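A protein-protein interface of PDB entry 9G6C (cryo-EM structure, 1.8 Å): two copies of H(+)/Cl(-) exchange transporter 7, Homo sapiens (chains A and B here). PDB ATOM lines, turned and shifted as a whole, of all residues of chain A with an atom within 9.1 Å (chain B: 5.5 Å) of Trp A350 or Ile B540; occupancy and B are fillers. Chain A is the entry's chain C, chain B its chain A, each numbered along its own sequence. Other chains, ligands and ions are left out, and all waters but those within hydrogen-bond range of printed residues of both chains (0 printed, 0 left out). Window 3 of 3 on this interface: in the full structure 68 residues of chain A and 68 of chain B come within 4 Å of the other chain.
Of chain B, only Ala B369 (3.7 Å), Thr B371 (3.5 Å), Ile B540 (3.9 Å) and Trp B541 (3.9 Å) come within 4 Å of Trp A350.
Of chain A, only Trp A350 (3.9 Å) comes within 4 Å of Ile B540.
Of the printed residues of chain A, Glu B366 touches Asp A351.
Printed residues of chain A within 4 Å of Trp B541: Trp A350 (3.9 Å).
Of the printed residues of chain A, Ala B369 touches Trp A350 (3.7 Å).
Of the printed residues of chain A, Thr B371 touches Trp A350.
Of the printed residues of chain A, Tyr B370 touches Leu A352 (3.6 Å).
Lys B546 touches none of the printed residues of chain A.
Ala B542 touches none of the printed residues of chain A.
The nearest residue of chain B that does not touch Trp A350 is Glu B366 (5.1 Å).
The nearest residue of chain A that does not touch Ile B540 is Asn A348 (8.4 Å).
Of the 12 printed residues of chain B, 6 touch a printed residue of chain A.
Hydrophobic or aromatic side chains of chain B within 4 Å of the printed part of chain A: Ala B369, Ile B540 and Trp B541.
Of the 13 printed residues of chain A, 3 touch a printed residue of chain B.
Hydrophobic or aromatic side chains of chain A that line the printed part of chain B: Trp A350 and Leu A352.
Among the printed residues, 6 pairs touch across the chains.
Among the printed residues, no Asp or Glu carboxylate lies within 4 Å of a Lys or Arg side-chain nitrogen of the other chain.
The backbone carbonyl oxygen (O) of Ala B369 lies within hydrogen-bond range of the side-chain amino group (NZ) of Lys B546, 2.9 Å away.
The side-chain amide nitrogen of Asn A339 sits at hydrogen-bond distance from the backbone carbonyl oxygen of Leu A352.
O of Trp B541 lies within hydrogen-bond range of NZ of Lys B546 (2.7 Å).
OD2 of Asp A351 is in hydrogen-bond range of OG of Ser A353.
Among the printed residues, merely in contact across the chains: Trp A350 with Ala B369 (3.7 Å), Trp A350 with Thr B371 (3.5 Å), Trp A350 with Ile B540 (3.9 Å), Trp A350 with Trp B541 (3.9 Å), Asp A351 with Glu B366 (3.8 Å) and Leu A352 with Tyr B370 (3.6 Å).
No position is printed for both chains.
Of the 6 pairs that touch across the chains among the printed residues, none has its exchanged pair printed and touching as well.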
ATOM      1  N   ASN A 339     -12.978  20.097  21.402  1.00  0.00           N
ATOM      2  CA  ASN A 339     -13.990  19.607  20.473  1.00  0.00           C
ATOM      3  C   ASN A 339     -14.395  18.173  20.799  1.00  0.00           C
ATOM      4  O   ASN A 339     -15.583  17.831  20.778  1.00  0.00           O
ATOM      5  CB  ASN A 339     -13.471  19.704  19.037  1.00  0.00           C
ATOM      6  CG  ASN A 339     -14.557  20.077  18.049  1.00  0.00           C
ATOM      7  OD1 ASN A 339     -15.747  19.960  18.343  1.00  0.00           O
ATOM      8  ND2 ASN A 339     -14.151  20.529  16.869  1.00  0.00           N
ATOM      9  N   PHE A 340     -13.416  17.318  21.096  1.00  0.00           N
ATOM     10  CA  PHE A 340     -13.703  15.902  21.301  1.00  0.00           C
ATOM     11  C   PHE A 340     -14.470  15.671  22.599  1.00  0.00           C
ATOM     12  O   PHE A 340     -15.437  14.903  22.630  1.00  0.00           O
ATOM     13  CB  PHE A 340     -12.400  15.101  21.290  1.00  0.00           C
ATOM     14  CG  PHE A 340     -12.576  13.653  21.639  1.00  0.00           C
ATOM     15  CD1 PHE A 340     -13.222  12.789  20.770  1.00  0.00           C
ATOM     16  CD2 PHE A 340     -12.085  13.151  22.833  1.00  0.00           C
ATOM     17  CE1 PHE A 340     -13.382  11.456  21.088  1.00  0.00           C
ATOM     18  CE2 PHE A 340     -12.241  11.818  23.156  1.00  0.00           C
ATOM     19  CZ  PHE A 340     -12.889  10.968  22.282  1.00  0.00           C
ATOM     20  N   LEU A 342     -16.263  17.895  24.420  1.00  0.00           N
ATOM     21  CA  LEU A 342     -17.590  18.503  24.361  1.00  0.00           C
ATOM     22  C   LEU A 342     -18.544  17.666  23.520  1.00  0.00           C
ATOM     23  O   LEU A 342     -19.739  17.577  23.826  1.00  0.00           O
ATOM     24  CB  LEU A 342     -17.502  19.926  23.810  1.00  0.00           C
ATOM     25  CG  LEU A 342     -17.123  21.028  24.800  1.00  0.00           C
ATOM     26  CD1 LEU A 342     -17.193  22.391  24.129  1.00  0.00           C
ATOM     27  CD2 LEU A 342     -18.017  20.982  26.026  1.00  0.00           C
ATOM     28  N   SER A 343     -18.037  17.052  22.449  1.00  0.00           N
ATOM     29  CA  SER A 343     -18.870  16.171  21.638  1.00  0.00           C
ATOM     30  C   SER A 343     -19.355  14.976  22.447  1.00  0.00           C
ATOM     31  O   SER A 343     -20.507  14.550  22.308  1.00  0.00           O
ATOM     32  CB  SER A 343     -18.096  15.709  20.402  1.00  0.00           C
ATOM     33  OG  SER A 343     -17.485  14.450  20.624  1.00  0.00           O
ATOM     34  N   ILE A 344     -18.487  14.417  23.292  1.00  0.00           N
ATOM     35  CA  ILE A 344     -18.903  13.338  24.183  1.00  0.00           C
ATOM     36  C   ILE A 344     -19.951  13.835  25.169  1.00  0.00           C
ATOM     37  O   ILE A 344     -20.955  13.160  25.425  1.00  0.00           O
ATOM     38  CB  ILE A 344     -17.681  12.744  24.909  1.00  0.00           C
ATOM     39  CG1 ILE A 344     -16.729  12.091  23.908  1.00  0.00           C
ATOM     40  CG2 ILE A 344     -18.120  11.738  25.960  1.00  0.00           C
ATOM     41  CD1 ILE A 344     -15.545  11.419  24.557  1.00  0.00           C
ATOM     42  N   HIS A 346     -22.031  16.310  24.808  1.00  0.00           N
ATOM     43  CA  HIS A 346     -23.267  16.577  24.083  1.00  0.00           C
ATOM     44  C   HIS A 346     -23.862  15.330  23.442  1.00  0.00           C
ATOM     45  O   HIS A 346     -24.917  15.425  22.808  1.00  0.00           O
ATOM     46  CB  HIS A 346     -23.030  17.643  23.010  1.00  0.00           C
ATOM     47  CG  HIS A 346     -22.722  18.999  23.562  1.00  0.00           C
ATOM     48  ND1 HIS A 346     -21.906  19.900  22.911  1.00  0.00           N
ATOM     49  CD2 HIS A 346     -23.119  19.608  24.704  1.00  0.00           C
ATOM     50  CE1 HIS A 346     -21.815  21.005  23.628  1.00  0.00           C
ATOM     51  NE2 HIS A 346     -22.542  20.854  24.721  1.00  0.00           N
ATOM     52  N   GLY A 347     -23.222  14.183  23.584  1.00  0.00           N
ATOM     53  CA  GLY A 347     -23.747  12.930  23.049  1.00  0.00           C
ATOM     54  C   GLY A 347     -23.275  12.530  21.668  1.00  0.00           C
ATOM     55  O   GLY A 347     -22.865  11.389  21.458  1.00  0.00           O
ATOM     56  N   ASN A 348     -23.326  13.458  20.715  1.00  0.00           N
ATOM     57  CA  ASN A 348     -22.937  13.175  19.333  1.00  0.00           C
ATOM     58  C   ASN A 348     -21.416  13.175  19.245  1.00  0.00           C
ATOM     59  O   ASN A 348     -20.783  14.200  18.989  1.00  0.00           O
ATOM     60  CB  ASN A 348     -23.550  14.191  18.379  1.00  0.00           C
ATOM     61  CG  ASN A 348     -23.743  13.633  16.983  1.00  0.00           C
ATOM     62  OD1 ASN A 348     -23.315  12.519  16.683  1.00  0.00           O
ATOM     63  ND2 ASN A 348     -24.389  14.409  16.120  1.00  0.00           N
ATOM     64  N   MET A 349     -20.822  12.000  19.461  1.00  0.00           N
ATOM     65  CA  MET A 349     -19.374  11.857  19.369  1.00  0.00           C
ATOM     66  C   MET A 349     -18.861  12.061  17.948  1.00  0.00           C
ATOM     67  O   MET A 349     -17.689  12.410  17.766  1.00  0.00           O
ATOM     68  CB  MET A 349     -18.959  10.479  19.889  1.00  0.00           C
ATOM     69  CG  MET A 349     -17.459  10.268  20.018  1.00  0.00           C
ATOM     70  SD  MET A 349     -17.027   9.271  21.457  1.00  0.00           S
ATOM     71  CE  MET A 349     -15.611   8.373  20.831  1.00  0.00           C
ATOM     72  N   TRP A 350     -19.713  11.871  16.943  1.00  0.00           N
ATOM     73  CA  TRP A 350     -19.316  11.974  15.546  1.00  0.00           C
ATOM     74  C   TRP A 350     -19.374  13.399  15.008  1.00  0.00           C
ATOM     75  O   TRP A 350     -18.990  13.625  13.857  1.00  0.00           O
ATOM     76  CB  TRP A 350     -20.204  11.070  14.684  1.00  0.00           C
ATOM     77  CG  TRP A 350     -19.462   9.978  13.976  1.00  0.00           C
ATOM     78  CD1 TRP A 350     -19.003  10.000  12.692  1.00  0.00           C
ATOM     79  CD2 TRP A 350     -19.105   8.697  14.509  1.00  0.00           C
ATOM     80  NE1 TRP A 350     -18.377   8.813  12.393  1.00  0.00           N
ATOM     81  CE2 TRP A 350     -18.426   7.997  13.493  1.00  0.00           C
ATOM     82  CE3 TRP A 350     -19.292   8.076  15.747  1.00  0.00           C
ATOM     83  CZ2 TRP A 350     -17.933   6.707  13.675  1.00  0.00           C
ATOM     84  CZ3 TRP A 350     -18.801   6.795  15.928  1.00  0.00           C
ATOM     85  CH2 TRP A 350     -18.130   6.125  14.897  1.00  0.00           C
ATOM     86  N   ASP A 351     -19.838  14.360  15.804  1.00  0.00           N
ATOM     87  CA  ASP A 351     -20.003  15.742  15.365  1.00  0.00           C
ATOM     88  C   ASP A 351     -19.007  16.620  16.111  1.00  0.00           C
ATOM     89  O   ASP A 351     -19.229  16.967  17.276  1.00  0.00           O
ATOM     90  CB  ASP A 351     -21.436  16.222  15.595  1.00  0.00           C
ATOM     91  CG  ASP A 351     -21.752  17.497  14.840  1.00  0.00           C
ATOM     92  OD1 ASP A 351     -21.170  17.707  13.755  1.00  0.00           O
ATOM     93  OD2 ASP A 351     -22.580  18.290  15.333  1.00  0.00           O
ATOM     94  N   LEU A 352     -17.914  16.980  15.440  1.00  0.00           N
ATOM     95  CA  LEU A 352     -16.903  17.869  16.015  1.00  0.00           C
ATOM     96  C   LEU A 352     -17.197  19.308  15.588  1.00  0.00           C
ATOM     97  O   LEU A 352     -16.478  19.928  14.802  1.00  0.00           O
ATOM     98  CB  LEU A 352     -15.507  17.429  15.595  1.00  0.00           C
ATOM     99  CG  LEU A 352     -15.067  16.034  16.045  1.00  0.00           C
ATOM    100  CD1 LEU A 352     -13.710  15.682  15.452  1.00  0.00           C
ATOM    101  CD2 LEU A 352     -15.032  15.943  17.560  1.00  0.00           C
ATOM    102  N   SER A 353     -18.290  19.837  16.133  1.00  0.00           N
ATOM    103  CA  SER A 353     -18.798  21.147  15.751  1.00  0.00           C
ATOM    104  C   SER A 353     -18.491  22.233  16.776  1.00  0.00           C
ATOM    105  O   SER A 353     -19.031  23.338  16.668  1.00  0.00           O
ATOM    106  CB  SER A 353     -20.308  21.074  15.511  1.00  0.00           C
ATOM    107  OG  SER A 353     -20.994  20.703  16.693  1.00  0.00           O
ATOM    108  N   GLU B 366     -20.964  15.617   7.148  1.00  0.00           N
ATOM    109  CA  GLU B 366     -20.887  14.486   8.066  1.00  0.00           C
ATOM    110  C   GLU B 366     -19.952  13.403   7.545  1.00  0.00           C
ATOM    111  O   GLU B 366     -19.275  12.736   8.336  1.00  0.00           O
ATOM    112  CB  GLU B 366     -22.282  13.911   8.314  1.00  0.00           C
ATOM    113  CG  GLU B 366     -23.334  14.948   8.677  1.00  0.00           C
ATOM    114  CD  GLU B 366     -22.793  16.040   9.583  1.00  0.00           C
ATOM    115  OE1 GLU B 366     -22.477  15.740  10.753  1.00  0.00           O
ATOM    116  OE2 GLU B 366     -22.683  17.196   9.122  1.00  0.00           O
ATOM    117  N   LYS B 367     -19.906  13.207   6.224  1.00  0.00           N
ATOM    118  CA  LYS B 367     -18.950  12.267   5.650  1.00  0.00           C
ATOM    119  C   LYS B 367     -17.519  12.683   5.960  1.00  0.00           C
ATOM    120  O   LYS B 367     -16.646  11.833   6.175  1.00  0.00           O
ATOM    121  CB  LYS B 367     -19.157  12.157   4.140  1.00  0.00           C
ATOM    122  CG  LYS B 367     -20.274  11.214   3.720  1.00  0.00           C
ATOM    123  CD  LYS B 367     -20.234  10.956   2.221  1.00  0.00           C
ATOM    124  CE  LYS B 367     -21.324   9.987   1.790  1.00  0.00           C
ATOM    125  NZ  LYS B 367     -21.152   8.641   2.402  1.00  0.00           N
ATOM    126  N   ALA B 369     -15.943  13.717   8.547  1.00  0.00           N
ATOM    127  CA  ALA B 369     -15.736  13.747   9.986  1.00  0.00           C
ATOM    128  C   ALA B 369     -14.940  12.518  10.399  1.00  0.00           C
ATOM    129  O   ALA B 369     -15.065  11.448   9.798  1.00  0.00           O
ATOM    130  CB  ALA B 369     -17.065  13.795  10.751  1.00  0.00           C
ATOM    131  N   TYR B 370     -14.118  12.678  11.434  1.00  0.00           N
ATOM    132  CA  TYR B 370     -13.238  11.613  11.885  1.00  0.00           C
ATOM    133  C   TYR B 370     -13.391  11.405  13.385  1.00  0.00           C
ATOM    134  O   TYR B 370     -13.837  12.292  14.118  1.00  0.00           O
ATOM    135  CB  TYR B 370     -11.769  11.911  11.546  1.00  0.00           C
ATOM    136  CG  TYR B 370     -11.209  13.140  12.226  1.00  0.00           C
ATOM    137  CD1 TYR B 370     -11.375  14.402  11.673  1.00  0.00           C
ATOM    138  CD2 TYR B 370     -10.501  13.034  13.416  1.00  0.00           C
ATOM    139  CE1 TYR B 370     -10.862  15.525  12.292  1.00  0.00           C
ATOM    140  CE2 TYR B 370      -9.983  14.151  14.041  1.00  0.00           C
ATOM    141  CZ  TYR B 370     -10.165  15.393  13.474  1.00  0.00           C
ATOM    142  OH  TYR B 370      -9.651  16.507  14.094  1.00  0.00           O
ATOM    143  N   THR B 371     -13.013  10.211  13.830  1.00  0.00           N
ATOM    144  CA  THR B 371     -13.025   9.834  15.236  1.00  0.00           C
ATOM    145  C   THR B 371     -11.595   9.618  15.716  1.00  0.00           C
ATOM    146  O   THR B 371     -10.635   9.719  14.948  1.00  0.00           O
ATOM    147  CB  THR B 371     -13.858   8.565  15.464  1.00  0.00           C
ATOM    148  OG1 THR B 371     -13.017   7.412  15.347  1.00  0.00           O
ATOM    149  CG2 THR B 371     -14.978   8.474  14.442  1.00  0.00           C
ATOM    150  N   ALA B 538     -18.292  -1.030   4.455  1.00  0.00           N
ATOM    151  CA  ALA B 538     -18.750   0.303   4.058  1.00  0.00           C
ATOM    152  C   ALA B 538     -19.201   1.119   5.269  1.00  0.00           C
ATOM    153  O   ALA B 538     -20.256   1.756   5.263  1.00  0.00           O
ATOM    154  CB  ALA B 538     -19.861   0.215   3.008  1.00  0.00           C
ATOM    155  N   ALA B 539     -18.385   1.091   6.322  1.00  0.00           N
ATOM    156  CA  ALA B 539     -18.667   1.888   7.507  1.00  0.00           C
ATOM    157  C   ALA B 539     -18.620   3.374   7.173  1.00  0.00           C
ATOM    158  O   ALA B 539     -17.848   3.818   6.319  1.00  0.00           O
ATOM    159  CB  ALA B 539     -17.672   1.561   8.619  1.00  0.00           C
ATOM    160  N   ILE B 540     -19.467   4.148   7.857  1.00  0.00           N
ATOM    161  CA  ILE B 540     -19.605   5.566   7.537  1.00  0.00           C
ATOM    162  C   ILE B 540     -18.318   6.329   7.825  1.00  0.00           C
ATOM    163  O   ILE B 540     -18.039   7.347   7.179  1.00  0.00           O
ATOM    164  CB  ILE B 540     -20.802   6.172   8.294  1.00  0.00           C
ATOM    165  CG1 ILE B 540     -20.581   6.095   9.807  1.00  0.00           C
ATOM    166  CG2 ILE B 540     -22.091   5.468   7.902  1.00  0.00           C
ATOM    167  CD1 ILE B 540     -21.354   7.135  10.587  1.00  0.00           C
ATOM    168  N   TRP B 541     -17.516   5.870   8.787  1.00  0.00           N
ATOM    169  CA  TRP B 541     -16.268   6.561   9.087  1.00  0.00           C
ATOM    170  C   TRP B 541     -15.200   6.308   8.030  1.00  0.00           C
ATOM    171  O   TRP B 541     -14.263   7.103   7.913  1.00  0.00           O
ATOM    172  CB  TRP B 541     -15.746   6.149  10.466  1.00  0.00           C
ATOM    173  CG  TRP B 541     -15.395   4.699  10.586  1.00  0.00           C
ATOM    174  CD1 TRP B 541     -16.213   3.689  11.002  1.00  0.00           C
ATOM    175  CD2 TRP B 541     -14.128   4.095  10.296  1.00  0.00           C
ATOM    176  NE1 TRP B 541     -15.535   2.494  10.986  1.00  0.00           N
ATOM    177  CE2 TRP B 541     -14.254   2.716  10.556  1.00  0.00           C
ATOM    178  CE3 TRP B 541     -12.902   4.586   9.839  1.00  0.00           C
ATOM    179  CZ2 TRP B 541     -13.200   1.824  10.375  1.00  0.00           C
ATOM    180  CZ3 TRP B 541     -11.857   3.699   9.660  1.00  0.00           C
ATOM    181  CH2 TRP B 541     -12.012   2.334   9.927  1.00  0.00           C
ATOM    182  N   ALA B 542     -15.322   5.228   7.262  1.00  0.00           N
ATOM    183  CA  ALA B 542     -14.351   4.906   6.216  1.00  0.00           C
ATOM    184  C   ALA B 542     -14.752   5.556   4.890  1.00  0.00           C
ATOM    185  O   ALA B 542     -15.002   4.895   3.883  1.00  0.00           O
ATOM    186  CB  ALA B 542     -14.211   3.395   6.076  1.00  0.00           C
ATOM    187  N   ASP B 543     -14.811   6.882   4.911  1.00  0.00           N
ATOM    188  CA  ASP B 543     -15.155   7.641   3.715  1.00  0.00           C
ATOM    189  C   ASP B 543     -13.917   7.810   2.843  1.00  0.00           C
ATOM    190  O   ASP B 543     -12.932   8.405   3.294  1.00  0.00           O
ATOM    191  CB  ASP B 543     -15.724   9.002   4.089  1.00  0.00           C
ATOM    192  CG  ASP B 543     -16.019   9.864   2.879  1.00  0.00           C
ATOM    193  OD1 ASP B 543     -16.959   9.534   2.126  1.00  0.00           O
ATOM    194  OD2 ASP B 543     -15.313  10.875   2.681  1.00  0.00           O
ATOM    195  N   LYS B 546     -12.352  11.443   2.490  1.00  0.00           N
ATOM    196  CA  LYS B 546     -11.571  11.941   3.617  1.00  0.00           C
ATOM    197  C   LYS B 546     -10.152  11.389   3.591  1.00  0.00           C
ATOM    198  O   LYS B 546      -9.189  12.115   3.863  1.00  0.00           O
ATOM    199  CB  LYS B 546     -12.264  11.580   4.931  1.00  0.00           C
ATOM    200  CG  LYS B 546     -11.468  11.931   6.175  1.00  0.00           C
ATOM    201  CD  LYS B 546     -12.172  11.451   7.434  1.00  0.00           C
ATOM    202  CE  LYS B 546     -12.701  10.036   7.263  1.00  0.00           C
ATOM    203  NZ  LYS B 546     -13.338   9.524   8.506  1.00  0.00           N
